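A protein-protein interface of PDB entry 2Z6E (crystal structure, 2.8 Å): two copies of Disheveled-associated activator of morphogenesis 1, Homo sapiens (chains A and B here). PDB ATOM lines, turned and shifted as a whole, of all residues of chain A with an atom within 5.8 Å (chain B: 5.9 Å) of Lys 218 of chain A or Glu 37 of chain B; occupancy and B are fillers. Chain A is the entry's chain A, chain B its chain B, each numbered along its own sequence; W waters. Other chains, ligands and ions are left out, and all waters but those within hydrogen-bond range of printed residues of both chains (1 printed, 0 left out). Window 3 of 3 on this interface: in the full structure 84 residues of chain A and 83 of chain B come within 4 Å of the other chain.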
ATOM      1  N   PHE A 212      10.773  25.806   0.294  1.00  0.00           N
ATOM      2  CA  PHE A 212       9.461  25.209   0.154  1.00  0.00           C
ATOM      3  C   PHE A 212       9.126  24.218   1.252  1.00  0.00           C
ATOM      4  O   PHE A 212       7.979  24.139   1.670  1.00  0.00           O
ATOM      5  CB  PHE A 212       9.372  24.489  -1.192  1.00  0.00           C
ATOM      6  CG  PHE A 212       8.005  23.963  -1.509  1.00  0.00           C
ATOM      7  CD1 PHE A 212       6.962  24.832  -1.804  1.00  0.00           C
ATOM      8  CD2 PHE A 212       7.755  22.599  -1.503  1.00  0.00           C
ATOM      9  CE1 PHE A 212       5.693  24.355  -2.085  1.00  0.00           C
ATOM     10  CE2 PHE A 212       6.482  22.108  -1.785  1.00  0.00           C
ATOM     11  CZ  PHE A 212       5.450  22.990  -2.076  1.00  0.00           C
ATOM     12  N   SER A 214      11.003  23.808   4.455  1.00  0.00           N
ATOM     13  CA  SER A 214      11.333  24.140   5.832  1.00  0.00           C
ATOM     14  C   SER A 214      10.154  24.363   6.764  1.00  0.00           C
ATOM     15  O   SER A 214       9.425  25.352   6.657  1.00  0.00           O
ATOM     16  CB  SER A 214      12.246  25.369   5.883  1.00  0.00           C
ATOM     17  OG  SER A 214      12.412  25.818   7.221  1.00  0.00           O
ATOM     18  N   GLY A 215       9.979  23.441   7.697  1.00  0.00           N
ATOM     19  CA  GLY A 215       8.917  23.584   8.667  1.00  0.00           C
ATOM     20  C   GLY A 215       9.349  24.635   9.672  1.00  0.00           C
ATOM     21  O   GLY A 215       8.512  25.257  10.315  1.00  0.00           O
ATOM     22  N   ALA A 216      10.656  24.842   9.822  1.00  0.00           N
ATOM     23  CA  ALA A 216      11.156  25.842  10.759  1.00  0.00           C
ATOM     24  C   ALA A 216      10.757  27.201  10.235  1.00  0.00           C
ATOM     25  O   ALA A 216      10.449  28.107  10.999  1.00  0.00           O
ATOM     26  CB  ALA A 216      12.669  25.760  10.874  1.00  0.00           C
ATOM     27  N   LEU A 217      10.768  27.335   8.911  1.00  0.00           N
ATOM     28  CA  LEU A 217      10.408  28.594   8.268  1.00  0.00           C
ATOM     29  C   LEU A 217       8.892  28.757   8.290  1.00  0.00           C
ATOM     30  O   LEU A 217       8.368  29.833   8.606  1.00  0.00           O
ATOM     31  CB  LEU A 217      10.934  28.627   6.833  1.00  0.00           C
ATOM     32  CG  LEU A 217      10.679  29.936   6.087  1.00  0.00           C
ATOM     33  CD1 LEU A 217      10.927  31.138   6.963  1.00  0.00           C
ATOM     34  CD2 LEU A 217      11.576  29.969   4.877  1.00  0.00           C
ATOM     35  N   LYS A 218       8.194  27.677   7.965  1.00  0.00           N
ATOM     36  CA  LYS A 218       6.746  27.685   7.965  1.00  0.00           C
ATOM     37  C   LYS A 218       6.261  28.132   9.342  1.00  0.00           C
ATOM     38  O   LYS A 218       5.475  29.069   9.447  1.00  0.00           O
ATOM     39  CB  LYS A 218       6.245  26.288   7.641  1.00  0.00           C
ATOM     40  CG  LYS A 218       4.823  26.205   7.174  1.00  0.00           C
ATOM     41  CD  LYS A 218       4.678  24.998   6.229  1.00  0.00           C
ATOM     42  CE  LYS A 218       3.221  24.674   5.884  1.00  0.00           C
ATOM     43  NZ  LYS A 218       2.440  24.166   7.063  1.00  0.00           N
ATOM     44  N   GLN A 219       6.758  27.502  10.402  1.00  0.00           N
ATOM     45  CA  GLN A 219       6.335  27.861  11.756  1.00  0.00           C
ATOM     46  C   GLN A 219       6.815  29.230  12.225  1.00  0.00           C
ATOM     47  O   GLN A 219       6.170  29.882  13.023  1.00  0.00           O
ATOM     48  CB  GLN A 219       6.797  26.801  12.763  1.00  0.00           C
ATOM     49  CG  GLN A 219       6.205  26.977  14.172  1.00  0.00           C
ATOM     50  CD  GLN A 219       4.668  26.987  14.171  1.00  0.00           C
ATOM     51  OE1 GLN A 219       4.022  26.029  13.723  1.00  0.00           O
ATOM     52  NE2 GLN A 219       4.081  28.077  14.672  1.00  0.00           N
ATOM     53  N   LEU A 220       7.950  29.677  11.735  1.00  0.00           N
ATOM     54  CA  LEU A 220       8.445  30.971  12.166  1.00  0.00           C
ATOM     55  C   LEU A 220       7.480  32.001  11.610  1.00  0.00           C
ATOM     56  O   LEU A 220       7.033  32.911  12.315  1.00  0.00           O
ATOM     57  CB  LEU A 220       9.864  31.186  11.623  1.00  0.00           C
ATOM     58  CG  LEU A 220      10.732  32.323  12.163  1.00  0.00           C
ATOM     59  CD1 LEU A 220      10.437  33.621  11.455  1.00  0.00           C
ATOM     60  CD2 LEU A 220      10.492  32.458  13.630  1.00  0.00           C
ATOM     61  N   LEU A 221       7.156  31.824  10.331  1.00  0.00           N
ATOM     62  CA  LEU A 221       6.238  32.694   9.615  1.00  0.00           C
ATOM     63  C   LEU A 221       4.909  32.788  10.363  1.00  0.00           C
ATOM     64  O   LEU A 221       4.390  33.882  10.579  1.00  0.00           O
ATOM     65  CB  LEU A 221       6.028  32.133   8.214  1.00  0.00           C
ATOM     66  CG  LEU A 221       6.602  32.875   7.005  1.00  0.00           C
ATOM     67  CD1 LEU A 221       7.668  33.873   7.424  1.00  0.00           C
ATOM     68  CD2 LEU A 221       7.152  31.855   6.011  1.00  0.00           C
ATOM     69  N   GLU A 222       4.370  31.646  10.783  1.00  0.00           N
ATOM     70  CA  GLU A 222       3.091  31.622  11.499  1.00  0.00           C
ATOM     71  C   GLU A 222       3.113  32.555  12.712  1.00  0.00           C
ATOM     72  O   GLU A 222       2.302  33.470  12.826  1.00  0.00           O
ATOM     73  CB  GLU A 222       2.771  30.189  11.935  1.00  0.00           C
ATOM     74  CG  GLU A 222       1.342  29.955  12.377  1.00  0.00           C
ATOM     75  CD  GLU A 222       0.987  28.470  12.439  1.00  0.00           C
ATOM     76  OE1 GLU A 222       0.959  27.806  11.380  1.00  0.00           O
ATOM     77  OE2 GLU A 222       0.735  27.960  13.547  1.00  0.00           O
ATOM     78  N   VAL A 223       4.060  32.334  13.610  1.00  0.00           N
ATOM     79  CA  VAL A 223       4.159  33.164  14.798  1.00  0.00           C
ATOM     80  C   VAL A 223       4.225  34.630  14.432  1.00  0.00           C
ATOM     81  O   VAL A 223       3.519  35.452  15.011  1.00  0.00           O
ATOM     82  CB  VAL A 223       5.415  32.819  15.625  1.00  0.00           C
ATOM     83  CG1 VAL A 223       5.528  33.766  16.812  1.00  0.00           C
ATOM     84  CG2 VAL A 223       5.357  31.377  16.103  1.00  0.00           C
ATOM     85  N   HIS A 366       5.092  30.077  -4.209  1.00  0.00           N
ATOM     86  CA  HIS A 366       4.763  29.618  -2.873  1.00  0.00           C
ATOM     87  C   HIS A 366       4.867  30.686  -1.819  1.00  0.00           C
ATOM     88  O   HIS A 366       4.264  30.557  -0.770  1.00  0.00           O
ATOM     89  CB  HIS A 366       5.630  28.439  -2.468  1.00  0.00           C
ATOM     90  CG  HIS A 366       5.097  27.681  -1.289  1.00  0.00           C
ATOM     91  ND1 HIS A 366       3.857  27.079  -1.291  1.00  0.00           N
ATOM     92  CD2 HIS A 366       5.641  27.420  -0.075  1.00  0.00           C
ATOM     93  CE1 HIS A 366       3.659  26.482  -0.130  1.00  0.00           C
ATOM     94  NE2 HIS A 366       4.726  26.672   0.625  1.00  0.00           N
ATOM     95  N   THR B  33      -0.443  29.282  -1.713  1.00  0.00           N
ATOM     96  CA  THR B  33       0.781  29.814  -1.127  1.00  0.00           C
ATOM     97  C   THR B  33       0.971  29.123   0.212  1.00  0.00           C
ATOM     98  O   THR B  33       0.160  28.285   0.594  1.00  0.00           O
ATOM     99  CB  THR B  33       0.677  31.292  -0.838  1.00  0.00           C
ATOM    100  OG1 THR B  33      -0.125  31.465   0.326  1.00  0.00           O
ATOM    101  CG2 THR B  33       0.043  32.025  -1.977  1.00  0.00           C
ATOM    102  N   VAL B  34       2.039  29.470   0.926  1.00  0.00           N
ATOM    103  CA  VAL B  34       2.277  28.868   2.228  1.00  0.00           C
ATOM    104  C   VAL B  34       1.127  29.206   3.134  1.00  0.00           C
ATOM    105  O   VAL B  34       0.612  28.340   3.839  1.00  0.00           O
ATOM    106  CB  VAL B  34       3.512  29.417   2.946  1.00  0.00           C
ATOM    107  CG1 VAL B  34       4.551  28.346   3.028  1.00  0.00           C
ATOM    108  CG2 VAL B  34       4.011  30.666   2.262  1.00  0.00           C
ATOM    109  N   TRP B  35       0.729  30.474   3.115  1.00  0.00           N
ATOM    110  CA  TRP B  35      -0.333  30.946   3.992  1.00  0.00           C
ATOM    111  C   TRP B  35      -1.612  30.090   4.017  1.00  0.00           C
ATOM    112  O   TRP B  35      -2.447  30.241   4.903  1.00  0.00           O
ATOM    113  CB  TRP B  35      -0.612  32.405   3.675  1.00  0.00           C
ATOM    114  CG  TRP B  35       0.669  33.174   3.568  1.00  0.00           C
ATOM    115  CD1 TRP B  35       1.319  33.546   2.416  1.00  0.00           C
ATOM    116  CD2 TRP B  35       1.486  33.636   4.650  1.00  0.00           C
ATOM    117  NE1 TRP B  35       2.492  34.221   2.717  1.00  0.00           N
ATOM    118  CE2 TRP B  35       2.616  34.288   4.080  1.00  0.00           C
ATOM    119  CE3 TRP B  35       1.379  33.564   6.045  1.00  0.00           C
ATOM    120  CZ2 TRP B  35       3.623  34.861   4.866  1.00  0.00           C
ATOM    121  CZ3 TRP B  35       2.381  34.133   6.825  1.00  0.00           C
ATOM    122  CH2 TRP B  35       3.484  34.774   6.235  1.00  0.00           C
ATOM    123  N   THR B  36      -1.744  29.170   3.068  1.00  0.00           N
ATOM    124  CA  THR B  36      -2.891  28.275   3.030  1.00  0.00           C
ATOM    125  C   THR B  36      -2.719  27.246   4.133  1.00  0.00           C
ATOM    126  O   THR B  36      -3.684  26.602   4.523  1.00  0.00           O
ATOM    127  CB  THR B  36      -2.990  27.510   1.682  1.00  0.00           C
ATOM    128  OG1 THR B  36      -3.475  28.395   0.668  1.00  0.00           O
ATOM    129  CG2 THR B  36      -3.919  26.290   1.797  1.00  0.00           C
ATOM    130  N   GLU B  37      -1.489  27.084   4.621  1.00  0.00           N
ATOM    131  CA  GLU B  37      -1.184  26.120   5.690  1.00  0.00           C
ATOM    132  C   GLU B  37      -0.778  26.784   6.997  1.00  0.00           C
ATOM    133  O   GLU B  37      -0.339  26.113   7.927  1.00  0.00           O
ATOM    134  CB  GLU B  37      -0.016  25.225   5.315  1.00  0.00           C
ATOM    135  CG  GLU B  37      -0.200  24.306   4.158  1.00  0.00           C
ATOM    136  CD  GLU B  37       1.033  23.450   3.983  1.00  0.00           C
ATOM    137  OE1 GLU B  37       1.264  22.569   4.851  1.00  0.00           O
ATOM    138  OE2 GLU B  37       1.777  23.678   2.997  1.00  0.00           O
ATOM    139  N   ILE B  38      -0.884  28.098   7.069  1.00  0.00           N
ATOM    140  CA  ILE B  38      -0.477  28.785   8.272  1.00  0.00           C
ATOM    141  C   ILE B  38      -1.688  29.402   8.907  1.00  0.00           C
ATOM    142  O   ILE B  38      -2.472  30.064   8.239  1.00  0.00           O
ATOM    143  CB  ILE B  38       0.561  29.868   7.937  1.00  0.00           C
ATOM    144  CG1 ILE B  38       1.818  29.195   7.379  1.00  0.00           C
ATOM    145  CG2 ILE B  38       0.874  30.703   9.164  1.00  0.00           C
ATOM    146  CD1 ILE B  38       2.840  30.136   6.789  1.00  0.00           C
ATOM    147  N   ASP B  39      -1.845  29.171  10.202  1.00  0.00           N
ATOM    148  CA  ASP B  39      -2.975  29.711  10.938  1.00  0.00           C
ATOM    149  C   ASP B  39      -2.518  30.331  12.231  1.00  0.00           C
ATOM    150  O   ASP B  39      -2.303  29.623  13.211  1.00  0.00           O
ATOM    151  CB  ASP B  39      -3.975  28.617  11.260  1.00  0.00           C
ATOM    152  CG  ASP B  39      -4.904  29.014  12.368  1.00  0.00           C
ATOM    153  OD1 ASP B  39      -5.228  30.218  12.445  1.00  0.00           O
ATOM    154  OD2 ASP B  39      -5.314  28.135  13.152  1.00  0.00           O
ATOM    155  N   LYS B  42      -3.514  29.224  15.907  1.00  0.00           N
ATOM    156  CA  LYS B  42      -2.770  28.216  16.648  1.00  0.00           C
ATOM    157  C   LYS B  42      -1.741  28.823  17.608  1.00  0.00           C
ATOM    158  O   LYS B  42      -1.467  28.274  18.669  1.00  0.00           O
ATOM    159  CB  LYS B  42      -2.043  27.276  15.675  1.00  0.00           C
ATOM    160  CG  LYS B  42      -2.949  26.620  14.655  1.00  0.00           C
ATOM    161  CD  LYS B  42      -2.542  25.193  14.357  1.00  0.00           C
ATOM    162  CE  LYS B  42      -1.210  25.108  13.631  1.00  0.00           C
ATOM    163  NZ  LYS B  42      -0.777  23.677  13.508  1.00  0.00           N
HETATM  164  O   HOH W   1       1.979  24.959   9.943  1.00  0.00           O
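Ile 38 of chain B touches Lys 218 of chain A.
CH2 of Trp 35 of chain B touches CG of Leu 221 of chain A (3.7 Å).
Glu 222 of chain A touches Ile 38 of chain B (CG to CG2, 3.3 Å).
Glu 222 of chain A touches Lys 42 of chain B.
O of His 366 of chain A touches CA of Thr 33 of chain B, 3.6 Å away.
Of the printed residues of chain B, Lys 218 of chain A touches Glu 37 and Ile 38.
Of the printed residues of chain B, Leu 221 of chain A touches Trp 35 (3.7 Å).
Of the printed residues of chain B, His 366 of chain A touches Thr 33 (3.6 Å) and Val 34 (2.9 Å).
Of the printed residues of chain A, Trp 35 of chain B touches Leu 221.
Of the printed residues of chain A, Val 34 of chain B touches His 366 (2.9 Å).
The nearest residue of chain B that does not touch Lys 218 of chain A is Val 34 of chain B (4.6 Å).
The nearest residue of chain A that does not touch Glu 37 of chain B is Glu 222 of chain A (4.1 Å).
The nearest printed residue of chain A that does not touch Ile 38 of chain B is Leu 221 of chain A (4.02 Å).
No position is printed for both chains.
Printed residues of chain A that touch a printed residue of chain B: Lys 218, Leu 221, Glu 222 and His 366.
Hydrophobic or aromatic side chains of chain A that line the printed part of chain B: Leu 221 and His 366.
Printed residues of chain B that touch a printed residue of chain A: Thr 33, Val 34, Trp 35, Glu 37, Ile 38, Asp 39 and Lys 42.
Among the printed residues, 8 pairs touch across the chains.
OE1 of Glu 222 of chain A lies within hydrogen-bond range of N of Asp 39 of chain B (3.3 Å).
The side-chain carboxylate (OE1) of Glu 37 of chain B lies within salt-bridge range of the side-chain amino group (NZ) of Lys 218 of chain A (3.0 Å).
The backbone carbonyl oxygen (O) of His 366 of chain A is in hydrogen-bond range of the backbone NH (N) of Val 34 of chain B (3.0 Å).
N of Lys 42 of chain B sits close to OD2 of Asp 39 of chain B (3.5 Å).
N of Trp 35 of chain B is in hydrogen-bond range of OG1 of Thr 33 of chain B (3.1 Å).
Water W1 lies within hydrogen-bond range of the side-chain amino group of Lys 218 of chain A (3.0 Å), the backbone carbonyl oxygen of Glu 37 of chain B (3.3 Å) and the side-chain carboxylate of Glu 222 of chain A (3.3 Å).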
